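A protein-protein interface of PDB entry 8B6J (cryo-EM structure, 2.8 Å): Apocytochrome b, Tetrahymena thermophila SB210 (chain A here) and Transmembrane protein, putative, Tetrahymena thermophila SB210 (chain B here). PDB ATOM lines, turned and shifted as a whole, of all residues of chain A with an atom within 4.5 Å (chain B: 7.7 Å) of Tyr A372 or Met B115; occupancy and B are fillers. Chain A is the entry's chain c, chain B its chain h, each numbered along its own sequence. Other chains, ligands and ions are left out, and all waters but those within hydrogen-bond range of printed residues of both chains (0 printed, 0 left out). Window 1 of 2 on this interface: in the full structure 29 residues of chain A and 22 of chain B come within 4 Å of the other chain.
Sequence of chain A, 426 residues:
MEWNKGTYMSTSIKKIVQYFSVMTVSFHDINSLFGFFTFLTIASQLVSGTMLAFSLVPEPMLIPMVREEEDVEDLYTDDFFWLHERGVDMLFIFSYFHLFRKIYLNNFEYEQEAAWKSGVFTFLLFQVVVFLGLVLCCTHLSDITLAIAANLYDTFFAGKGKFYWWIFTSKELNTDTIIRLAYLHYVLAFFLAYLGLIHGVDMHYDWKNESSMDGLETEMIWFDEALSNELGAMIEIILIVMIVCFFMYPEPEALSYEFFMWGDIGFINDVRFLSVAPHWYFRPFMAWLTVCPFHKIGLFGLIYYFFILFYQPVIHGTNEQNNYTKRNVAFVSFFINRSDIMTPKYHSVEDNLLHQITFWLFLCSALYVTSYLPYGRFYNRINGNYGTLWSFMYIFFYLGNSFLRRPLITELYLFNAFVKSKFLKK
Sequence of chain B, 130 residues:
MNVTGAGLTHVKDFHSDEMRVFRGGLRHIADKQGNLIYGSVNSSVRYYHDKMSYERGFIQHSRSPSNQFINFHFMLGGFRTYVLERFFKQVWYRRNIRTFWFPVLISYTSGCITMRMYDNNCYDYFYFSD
The backbone carbonyl oxygen (O) of Pro A374 sits at hydrogen-bond distance from the side-chain hydroxyl (OH) of Tyr B118, at 2.8 Å. OG1 of Thr B114 lies close to OD1 of Asn A385 (3.4 Å). OH of Tyr A368 sits at hydrogen-bond distance from OG1 of Thr B114 (2.9 Å).
The side-chain hydroxyl (OH) of Tyr A379 sits at hydrogen-bond distance from the backbone carbonyl oxygen (O) of Asn A385, 3.2 Å away. O of Ser B110 is in hydrogen-bond range of OG1 of Thr B114 (3.0 Å). The side-chain hydroxyl (OH) of Tyr A372 sits close to the side-chain amide nitrogen (ND2) of Asn A385 (3.2 Å). OD1 of Asn A385 sits at hydrogen-bond distance from N of Thr A388 (3.3 Å). The side-chain hydroxyl (OH) of Tyr A368 is in hydrogen-bond range of the side-chain amide nitrogen (ND2) of Asn A385, 2.4 Å away. The side-chain hydroxyl of Tyr A372 is in hydrogen-bond range of the side-chain hydroxyl of Thr A388 (2.7 Å).
Among the printed residues, merely in contact across the chains: Tyr A368 with Gly B111 (3.4 Å), Tyr A368 with Met B115 (3.7 Å), Tyr A372 with Met B115 (3.4 Å), Tyr A379 with Tyr B118 (3.6 Å), Asn A385 with Met B115 (3.5 Å) and Asn A385 with Tyr B118 (3.8 Å).
Val A369 touches none of the printed residues of chain B. Tyr A372 touches just one residue of chain B: Met B115 (3.4 Å). Printed residues of chain B within 4 Å of Asn A385: Thr B114, Met B115 and Tyr B118. Of the printed residues of chain A, Gly B111 touches Tyr A368 (3.4 Å). Printed residues of chain A within 4 Å of Thr B114: Tyr A368 and Asn A385. Met B115 touches just these residues of chain A: Tyr A368, Tyr A372 and Asn A385. Of the printed residues of chain A, Tyr B118 touches Pro A374, Tyr A379 and Asn A385. Cys B122 touches none of the printed residues of chain A. The nearest residue of chain B that does not touch Tyr A372 is Tyr B118 (4.1 Å). The nearest printed residue of chain B that does not touch Asn A385 is Gly B111 (5.2 Å).
Of the 12 printed residues of chain A, 5 touch a printed residue of chain B. Among the printed residues, no Asp or Glu carboxylate lies within 4 Å of a Lys or Arg side-chain nitrogen of the other chain.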
ATOM      1  N   ARG A 283      18.259 -24.816 -14.320  1.00  0.00           N
ATOM      2  CA  ARG A 283      17.736 -23.663 -13.595  1.00  0.00           C
ATOM      3  C   ARG A 283      18.350 -22.344 -14.046  1.00  0.00           C
ATOM      4  O   ARG A 283      17.595 -21.368 -14.198  1.00  0.00           O
ATOM      5  CB  ARG A 283      17.959 -23.872 -12.095  1.00  0.00           C
ATOM      6  CG  ARG A 283      17.452 -22.751 -11.215  1.00  0.00           C
ATOM      7  CD  ARG A 283      17.761 -23.048  -9.761  1.00  0.00           C
ATOM      8  NE  ARG A 283      17.126 -24.282  -9.313  1.00  0.00           N
ATOM      9  CZ  ARG A 283      17.514 -24.986  -8.259  1.00  0.00           C
ATOM     10  NH1 ARG A 283      18.552 -24.620  -7.526  1.00  0.00           N
ATOM     11  NH2 ARG A 283      16.848 -26.091  -7.938  1.00  0.00           N
ATOM     12  N   ALA A 287      16.128 -19.142 -15.349  1.00  0.00           N
ATOM     13  CA  ALA A 287      16.260 -17.901 -14.595  1.00  0.00           C
ATOM     14  C   ALA A 287      16.657 -16.748 -15.504  1.00  0.00           C
ATOM     15  O   ALA A 287      16.152 -15.631 -15.357  1.00  0.00           O
ATOM     16  CB  ALA A 287      17.283 -18.077 -13.474  1.00  0.00           C
ATOM     17  N   TYR A 368      25.431 -18.245  -7.610  1.00  0.00           N
ATOM     18  CA  TYR A 368      24.254 -17.462  -7.253  1.00  0.00           C
ATOM     19  C   TYR A 368      23.193 -17.550  -8.338  1.00  0.00           C
ATOM     20  O   TYR A 368      21.994 -17.604  -8.043  1.00  0.00           O
ATOM     21  CB  TYR A 368      24.646 -16.008  -7.005  1.00  0.00           C
ATOM     22  CG  TYR A 368      23.524 -15.174  -6.438  1.00  0.00           C
ATOM     23  CD1 TYR A 368      23.259 -15.170  -5.079  1.00  0.00           C
ATOM     24  CD2 TYR A 368      22.726 -14.397  -7.261  1.00  0.00           C
ATOM     25  CE1 TYR A 368      22.236 -14.416  -4.554  1.00  0.00           C
ATOM     26  CE2 TYR A 368      21.700 -13.638  -6.745  1.00  0.00           C
ATOM     27  CZ  TYR A 368      21.458 -13.651  -5.391  1.00  0.00           C
ATOM     28  OH  TYR A 368      20.436 -12.896  -4.867  1.00  0.00           O
ATOM     29  N   VAL A 369      23.615 -17.564  -9.602  1.00  0.00           N
ATOM     30  CA  VAL A 369      22.664 -17.698 -10.700  1.00  0.00           C
ATOM     31  C   VAL A 369      21.926 -19.025 -10.600  1.00  0.00           C
ATOM     32  O   VAL A 369      20.712 -19.096 -10.826  1.00  0.00           O
ATOM     33  CB  VAL A 369      23.390 -17.549 -12.049  1.00  0.00           C
ATOM     34  CG1 VAL A 369      22.494 -17.987 -13.178  1.00  0.00           C
ATOM     35  CG2 VAL A 369      23.824 -16.113 -12.252  1.00  0.00           C
ATOM     36  N   THR A 370      22.640 -20.097 -10.261  1.00  0.00           N
ATOM     37  CA  THR A 370      21.986 -21.391 -10.079  1.00  0.00           C
ATOM     38  C   THR A 370      21.338 -21.544  -8.708  1.00  0.00           C
ATOM     39  O   THR A 370      20.767 -22.603  -8.429  1.00  0.00           O
ATOM     40  CB  THR A 370      22.983 -22.533 -10.283  1.00  0.00           C
ATOM     41  OG1 THR A 370      24.061 -22.407  -9.348  1.00  0.00           O
ATOM     42  CG2 THR A 370      23.529 -22.511 -11.690  1.00  0.00           C
ATOM     43  N   SER A 371      21.413 -20.525  -7.850  1.00  0.00           N
ATOM     44  CA  SER A 371      20.980 -20.685  -6.466  1.00  0.00           C
ATOM     45  C   SER A 371      19.465 -20.798  -6.328  1.00  0.00           C
ATOM     46  O   SER A 371      18.987 -21.464  -5.404  1.00  0.00           O
ATOM     47  CB  SER A 371      21.493 -19.518  -5.624  1.00  0.00           C
ATOM     48  OG  SER A 371      20.924 -18.294  -6.050  1.00  0.00           O
ATOM     49  N   TYR A 372      18.689 -20.156  -7.199  1.00  0.00           N
ATOM     50  CA  TYR A 372      17.244 -20.124  -7.002  1.00  0.00           C
ATOM     51  C   TYR A 372      16.549 -19.776  -8.311  1.00  0.00           C
ATOM     52  O   TYR A 372      17.184 -19.415  -9.304  1.00  0.00           O
ATOM     53  CB  TYR A 372      16.861 -19.117  -5.916  1.00  0.00           C
ATOM     54  CG  TYR A 372      16.840 -17.691  -6.410  1.00  0.00           C
ATOM     55  CD1 TYR A 372      18.016 -17.027  -6.722  1.00  0.00           C
ATOM     56  CD2 TYR A 372      15.645 -17.011  -6.570  1.00  0.00           C
ATOM     57  CE1 TYR A 372      18.001 -15.728  -7.178  1.00  0.00           C
ATOM     58  CE2 TYR A 372      15.619 -15.711  -7.024  1.00  0.00           C
ATOM     59  CZ  TYR A 372      16.799 -15.075  -7.326  1.00  0.00           C
ATOM     60  OH  TYR A 372      16.776 -13.778  -7.779  1.00  0.00           O
ATOM     61  N   LEU A 373      15.199 -19.896  -8.291  1.00  0.00           N
ATOM     62  CA  LEU A 373      14.320 -19.536  -9.402  1.00  0.00           C
ATOM     63  C   LEU A 373      13.824 -18.103  -9.237  1.00  0.00           C
ATOM     64  O   LEU A 373      13.279 -17.765  -8.180  1.00  0.00           O
ATOM     65  CB  LEU A 373      13.121 -20.473  -9.477  1.00  0.00           C
ATOM     66  CG  LEU A 373      13.290 -21.778 -10.256  1.00  0.00           C
ATOM     67  CD1 LEU A 373      13.585 -21.504 -11.722  1.00  0.00           C
ATOM     68  CD2 LEU A 373      14.379 -22.627  -9.633  1.00  0.00           C
ATOM     69  N   PRO A 374      13.974 -17.241 -10.246  1.00  0.00           N
ATOM     70  CA  PRO A 374      13.474 -15.864 -10.108  1.00  0.00           C
ATOM     71  C   PRO A 374      11.975 -15.760  -9.874  1.00  0.00           C
ATOM     72  O   PRO A 374      11.514 -14.702  -9.428  1.00  0.00           O
ATOM     73  CB  PRO A 374      13.881 -15.216 -11.436  1.00  0.00           C
ATOM     74  CG  PRO A 374      15.090 -15.961 -11.841  1.00  0.00           C
ATOM     75  CD  PRO A 374      14.836 -17.382 -11.430  1.00  0.00           C
ATOM     76  N   TYR A 379       8.356 -11.302 -10.562  1.00  0.00           N
ATOM     77  CA  TYR A 379       9.767 -10.964 -10.431  1.00  0.00           C
ATOM     78  C   TYR A 379      10.102  -9.619 -11.057  1.00  0.00           C
ATOM     79  O   TYR A 379      11.108  -9.010 -10.682  1.00  0.00           O
ATOM     80  CB  TYR A 379      10.627 -12.057 -11.067  1.00  0.00           C
ATOM     81  CG  TYR A 379      12.109 -11.771 -11.021  1.00  0.00           C
ATOM     82  CD1 TYR A 379      12.869 -12.121  -9.915  1.00  0.00           C
ATOM     83  CD2 TYR A 379      12.749 -11.153 -12.085  1.00  0.00           C
ATOM     84  CE1 TYR A 379      14.222 -11.862  -9.870  1.00  0.00           C
ATOM     85  CE2 TYR A 379      14.100 -10.889 -12.048  1.00  0.00           C
ATOM     86  CZ  TYR A 379      14.833 -11.246 -10.940  1.00  0.00           C
ATOM     87  OH  TYR A 379      16.181 -10.983 -10.902  1.00  0.00           O
ATOM     88  N   ASN A 385      15.613  -9.272  -8.068  1.00  0.00           N
ATOM     89  CA  ASN A 385      16.850  -9.446  -7.323  1.00  0.00           C
ATOM     90  C   ASN A 385      18.016  -8.840  -8.089  1.00  0.00           C
ATOM     91  O   ASN A 385      18.361  -9.299  -9.180  1.00  0.00           O
ATOM     92  CB  ASN A 385      17.087 -10.938  -7.077  1.00  0.00           C
ATOM     93  CG  ASN A 385      18.273 -11.208  -6.174  1.00  0.00           C
ATOM     94  OD1 ASN A 385      19.272 -10.493  -6.208  1.00  0.00           O
ATOM     95  ND2 ASN A 385      18.169 -12.251  -5.363  1.00  0.00           N
ATOM     96  N   THR A 388      20.999 -11.266  -8.959  1.00  0.00           N
ATOM     97  CA  THR A 388      20.909 -12.102 -10.150  1.00  0.00           C
ATOM     98  C   THR A 388      21.385 -11.344 -11.384  1.00  0.00           C
ATOM     99  O   THR A 388      22.149 -11.874 -12.200  1.00  0.00           O
ATOM    100  CB  THR A 388      19.473 -12.590 -10.340  1.00  0.00           C
ATOM    101  OG1 THR A 388      19.029 -13.253  -9.151  1.00  0.00           O
ATOM    102  CG2 THR A 388      19.381 -13.554 -11.511  1.00  0.00           C
ATOM    103  N   THR B 109      28.159 -12.411   0.870  1.00  0.00           N
ATOM    104  CA  THR B 109      27.447 -11.365   1.595  1.00  0.00           C
ATOM    105  C   THR B 109      26.531 -10.574   0.669  1.00  0.00           C
ATOM    106  O   THR B 109      25.385 -10.274   1.025  1.00  0.00           O
ATOM    107  CB  THR B 109      28.446 -10.434   2.280  1.00  0.00           C
ATOM    108  OG1 THR B 109      29.277 -11.191   3.167  1.00  0.00           O
ATOM    109  CG2 THR B 109      27.721  -9.354   3.067  1.00  0.00           C
ATOM    110  N   SER B 110      27.017 -10.225  -0.526  1.00  0.00           N
ATOM    111  CA  SER B 110      26.192  -9.462  -1.455  1.00  0.00           C
ATOM    112  C   SER B 110      24.974 -10.263  -1.892  1.00  0.00           C
ATOM    113  O   SER B 110      23.865  -9.724  -1.979  1.00  0.00           O
ATOM    114  CB  SER B 110      27.023  -9.044  -2.666  1.00  0.00           C
ATOM    115  OG  SER B 110      28.126  -8.247  -2.273  1.00  0.00           O
ATOM    116  N   GLY B 111      25.161 -11.553  -2.180  1.00  0.00           N
ATOM    117  CA  GLY B 111      24.030 -12.386  -2.545  1.00  0.00           C
ATOM    118  C   GLY B 111      23.026 -12.514  -1.420  1.00  0.00           C
ATOM    119  O   GLY B 111      21.816 -12.457  -1.647  1.00  0.00           O
ATOM    120  N   CYS B 112      23.512 -12.678  -0.188  1.00  0.00           N
ATOM    121  CA  CYS B 112      22.613 -12.733   0.957  1.00  0.00           C
ATOM    122  C   CYS B 112      21.796 -11.451   1.073  1.00  0.00           C
ATOM    123  O   CYS B 112      20.575 -11.493   1.257  1.00  0.00           O
ATOM    124  CB  CYS B 112      23.420 -12.982   2.232  1.00  0.00           C
ATOM    125  SG  CYS B 112      22.603 -12.464   3.757  1.00  0.00           S
ATOM    126  N   ILE B 113      22.456 -10.298   0.950  1.00  0.00           N
ATOM    127  CA  ILE B 113      21.752  -9.024   1.097  1.00  0.00           C
ATOM    128  C   ILE B 113      20.726  -8.846  -0.014  1.00  0.00           C
ATOM    129  O   ILE B 113      19.587  -8.424   0.233  1.00  0.00           O
ATOM    130  CB  ILE B 113      22.758  -7.859   1.128  1.00  0.00           C
ATOM    131  CG1 ILE B 113      23.664  -7.958   2.360  1.00  0.00           C
ATOM    132  CG2 ILE B 113      22.029  -6.524   1.106  1.00  0.00           C
ATOM    133  CD1 ILE B 113      22.944  -7.807   3.686  1.00  0.00           C
ATOM    134  N   THR B 114      21.109  -9.144  -1.258  1.00  0.00           N
ATOM    135  CA  THR B 114      20.184  -8.969  -2.373  1.00  0.00           C
ATOM    136  C   THR B 114      18.995  -9.913  -2.255  1.00  0.00           C
ATOM    137  O   THR B 114      17.854  -9.522  -2.532  1.00  0.00           O
ATOM    138  CB  THR B 114      20.908  -9.179  -3.701  1.00  0.00           C
ATOM    139  OG1 THR B 114      21.569 -10.450  -3.698  1.00  0.00           O
ATOM    140  CG2 THR B 114      21.929  -8.078  -3.932  1.00  0.00           C
ATOM    141  N   MET B 115      19.235 -11.161  -1.843  1.00  0.00           N
ATOM    142  CA  MET B 115      18.132 -12.092  -1.646  1.00  0.00           C
ATOM    143  C   MET B 115      17.215 -11.622  -0.526  1.00  0.00           C
ATOM    144  O   MET B 115      15.993 -11.774  -0.614  1.00  0.00           O
ATOM    145  CB  MET B 115      18.672 -13.489  -1.347  1.00  0.00           C
ATOM    146  CG  MET B 115      17.592 -14.537  -1.115  1.00  0.00           C
ATOM    147  SD  MET B 115      16.489 -14.768  -2.519  1.00  0.00           S
ATOM    148  CE  MET B 115      17.638 -15.356  -3.753  1.00  0.00           C
ATOM    149  N   ARG B 116      17.783 -11.061   0.543  1.00  0.00           N
ATOM    150  CA  ARG B 116      16.947 -10.534   1.617  1.00  0.00           C
ATOM    151  C   ARG B 116      16.084  -9.380   1.128  1.00  0.00           C
ATOM    152  O   ARG B 116      14.904  -9.288   1.483  1.00  0.00           O
ATOM    153  CB  ARG B 116      17.814 -10.090   2.795  1.00  0.00           C
ATOM    154  CG  ARG B 116      18.108 -11.196   3.791  1.00  0.00           C
ATOM    155  CD  ARG B 116      16.879 -11.555   4.613  1.00  0.00           C
ATOM    156  NE  ARG B 116      17.091 -12.761   5.403  1.00  0.00           N
ATOM    157  CZ  ARG B 116      16.219 -13.253   6.272  1.00  0.00           C
ATOM    158  NH1 ARG B 116      15.060 -12.658   6.500  1.00  0.00           N
ATOM    159  NH2 ARG B 116      16.517 -14.368   6.930  1.00  0.00           N
ATOM    160  N   MET B 117      16.653  -8.480   0.326  1.00  0.00           N
ATOM    161  CA  MET B 117      15.858  -7.379  -0.213  1.00  0.00           C
ATOM    162  C   MET B 117      14.748  -7.900  -1.120  1.00  0.00           C
ATOM    163  O   MET B 117      13.609  -7.415  -1.073  1.00  0.00           O
ATOM    164  CB  MET B 117      16.759  -6.406  -0.970  1.00  0.00           C
ATOM    165  CG  MET B 117      17.791  -5.716  -0.094  1.00  0.00           C
ATOM    166  SD  MET B 117      18.896  -4.639  -1.023  1.00  0.00           S
ATOM    167  CE  MET B 117      17.763  -3.355  -1.542  1.00  0.00           C
ATOM    168  N   TYR B 118      15.064  -8.894  -1.952  1.00  0.00           N
ATOM    169  CA  TYR B 118      14.057  -9.501  -2.816  1.00  0.00           C
ATOM    170  C   TYR B 118      12.936 -10.134  -1.996  1.00  0.00           C
ATOM    171  O   TYR B 118      11.751  -9.958  -2.305  1.00  0.00           O
ATOM    172  CB  TYR B 118      14.737 -10.531  -3.718  1.00  0.00           C
ATOM    173  CG  TYR B 118      13.813 -11.389  -4.547  1.00  0.00           C
ATOM    174  CD1 TYR B 118      13.135 -10.866  -5.635  1.00  0.00           C
ATOM    175  CD2 TYR B 118      13.648 -12.735  -4.260  1.00  0.00           C
ATOM    176  CE1 TYR B 118      12.300 -11.654  -6.400  1.00  0.00           C
ATOM    177  CE2 TYR B 118      12.818 -13.529  -5.018  1.00  0.00           C
ATOM    178  CZ  TYR B 118      12.147 -12.986  -6.087  1.00  0.00           C
ATOM    179  OH  TYR B 118      11.319 -13.780  -6.843  1.00  0.00           O
ATOM    180  N   ASP B 119      13.293 -10.856  -0.933  1.00  0.00           N
ATOM    181  CA  ASP B 119      12.286 -11.480  -0.082  1.00  0.00           C
ATOM    182  C   ASP B 119      11.452 -10.438   0.650  1.00  0.00           C
ATOM    183  O   ASP B 119      10.254 -10.637   0.862  1.00  0.00           O
ATOM    184  CB  ASP B 119      12.953 -12.422   0.917  1.00  0.00           C
ATOM    185  CG  ASP B 119      13.538 -13.648   0.256  1.00  0.00           C
ATOM    186  OD1 ASP B 119      13.403 -13.781  -0.977  1.00  0.00           O
ATOM    187  OD2 ASP B 119      14.131 -14.483   0.970  1.00  0.00           O
ATOM    188  N   ASN B 120      12.066  -9.328   1.063  1.00  0.00           N
ATOM    189  CA  ASN B 120      11.304  -8.273   1.720  1.00  0.00           C
ATOM    190  C   ASN B 120      10.311  -7.633   0.758  1.00  0.00           C
ATOM    191  O   ASN B 120       9.176  -7.324   1.141  1.00  0.00           O
ATOM    192  CB  ASN B 120      12.251  -7.224   2.298  1.00  0.00           C
ATOM    193  CG  ASN B 120      13.118  -7.775   3.411  1.00  0.00           C
ATOM    194  OD1 ASN B 120      12.774  -8.774   4.042  1.00  0.00           O
ATOM    195  ND2 ASN B 120      14.247  -7.125   3.660  1.00  0.00           N
ATOM    196  N   ASN B 121      10.717  -7.426  -0.497  1.00  0.00           N
ATOM    197  CA  ASN B 121       9.769  -6.934  -1.493  1.00  0.00           C
ATOM    198  C   ASN B 121       8.640  -7.934  -1.707  1.00  0.00           C
ATOM    199  O   ASN B 121       7.471  -7.548  -1.838  1.00  0.00           O
ATOM    200  CB  ASN B 121      10.486  -6.647  -2.810  1.00  0.00           C
ATOM    201  CG  ASN B 121      11.382  -5.432  -2.732  1.00  0.00           C
ATOM    202  OD1 ASN B 121      11.080  -4.467  -2.031  1.00  0.00           O
ATOM    203  ND2 ASN B 121      12.495  -5.470  -3.456  1.00  0.00           N
ATOM    204  N   CYS B 122       8.970  -9.226  -1.742  1.00  0.00           N
ATOM    205  CA  CYS B 122       7.937 -10.250  -1.870  1.00  0.00           C
ATOM    206  C   CYS B 122       6.971 -10.207  -0.691  1.00  0.00           C
ATOM    207  O   CYS B 122       5.755 -10.353  -0.867  1.00  0.00           O
ATOM    208  CB  CYS B 122       8.588 -11.628  -1.980  1.00  0.00           C
ATOM    209  SG  CYS B 122       7.421 -12.998  -1.972  1.00  0.00           S
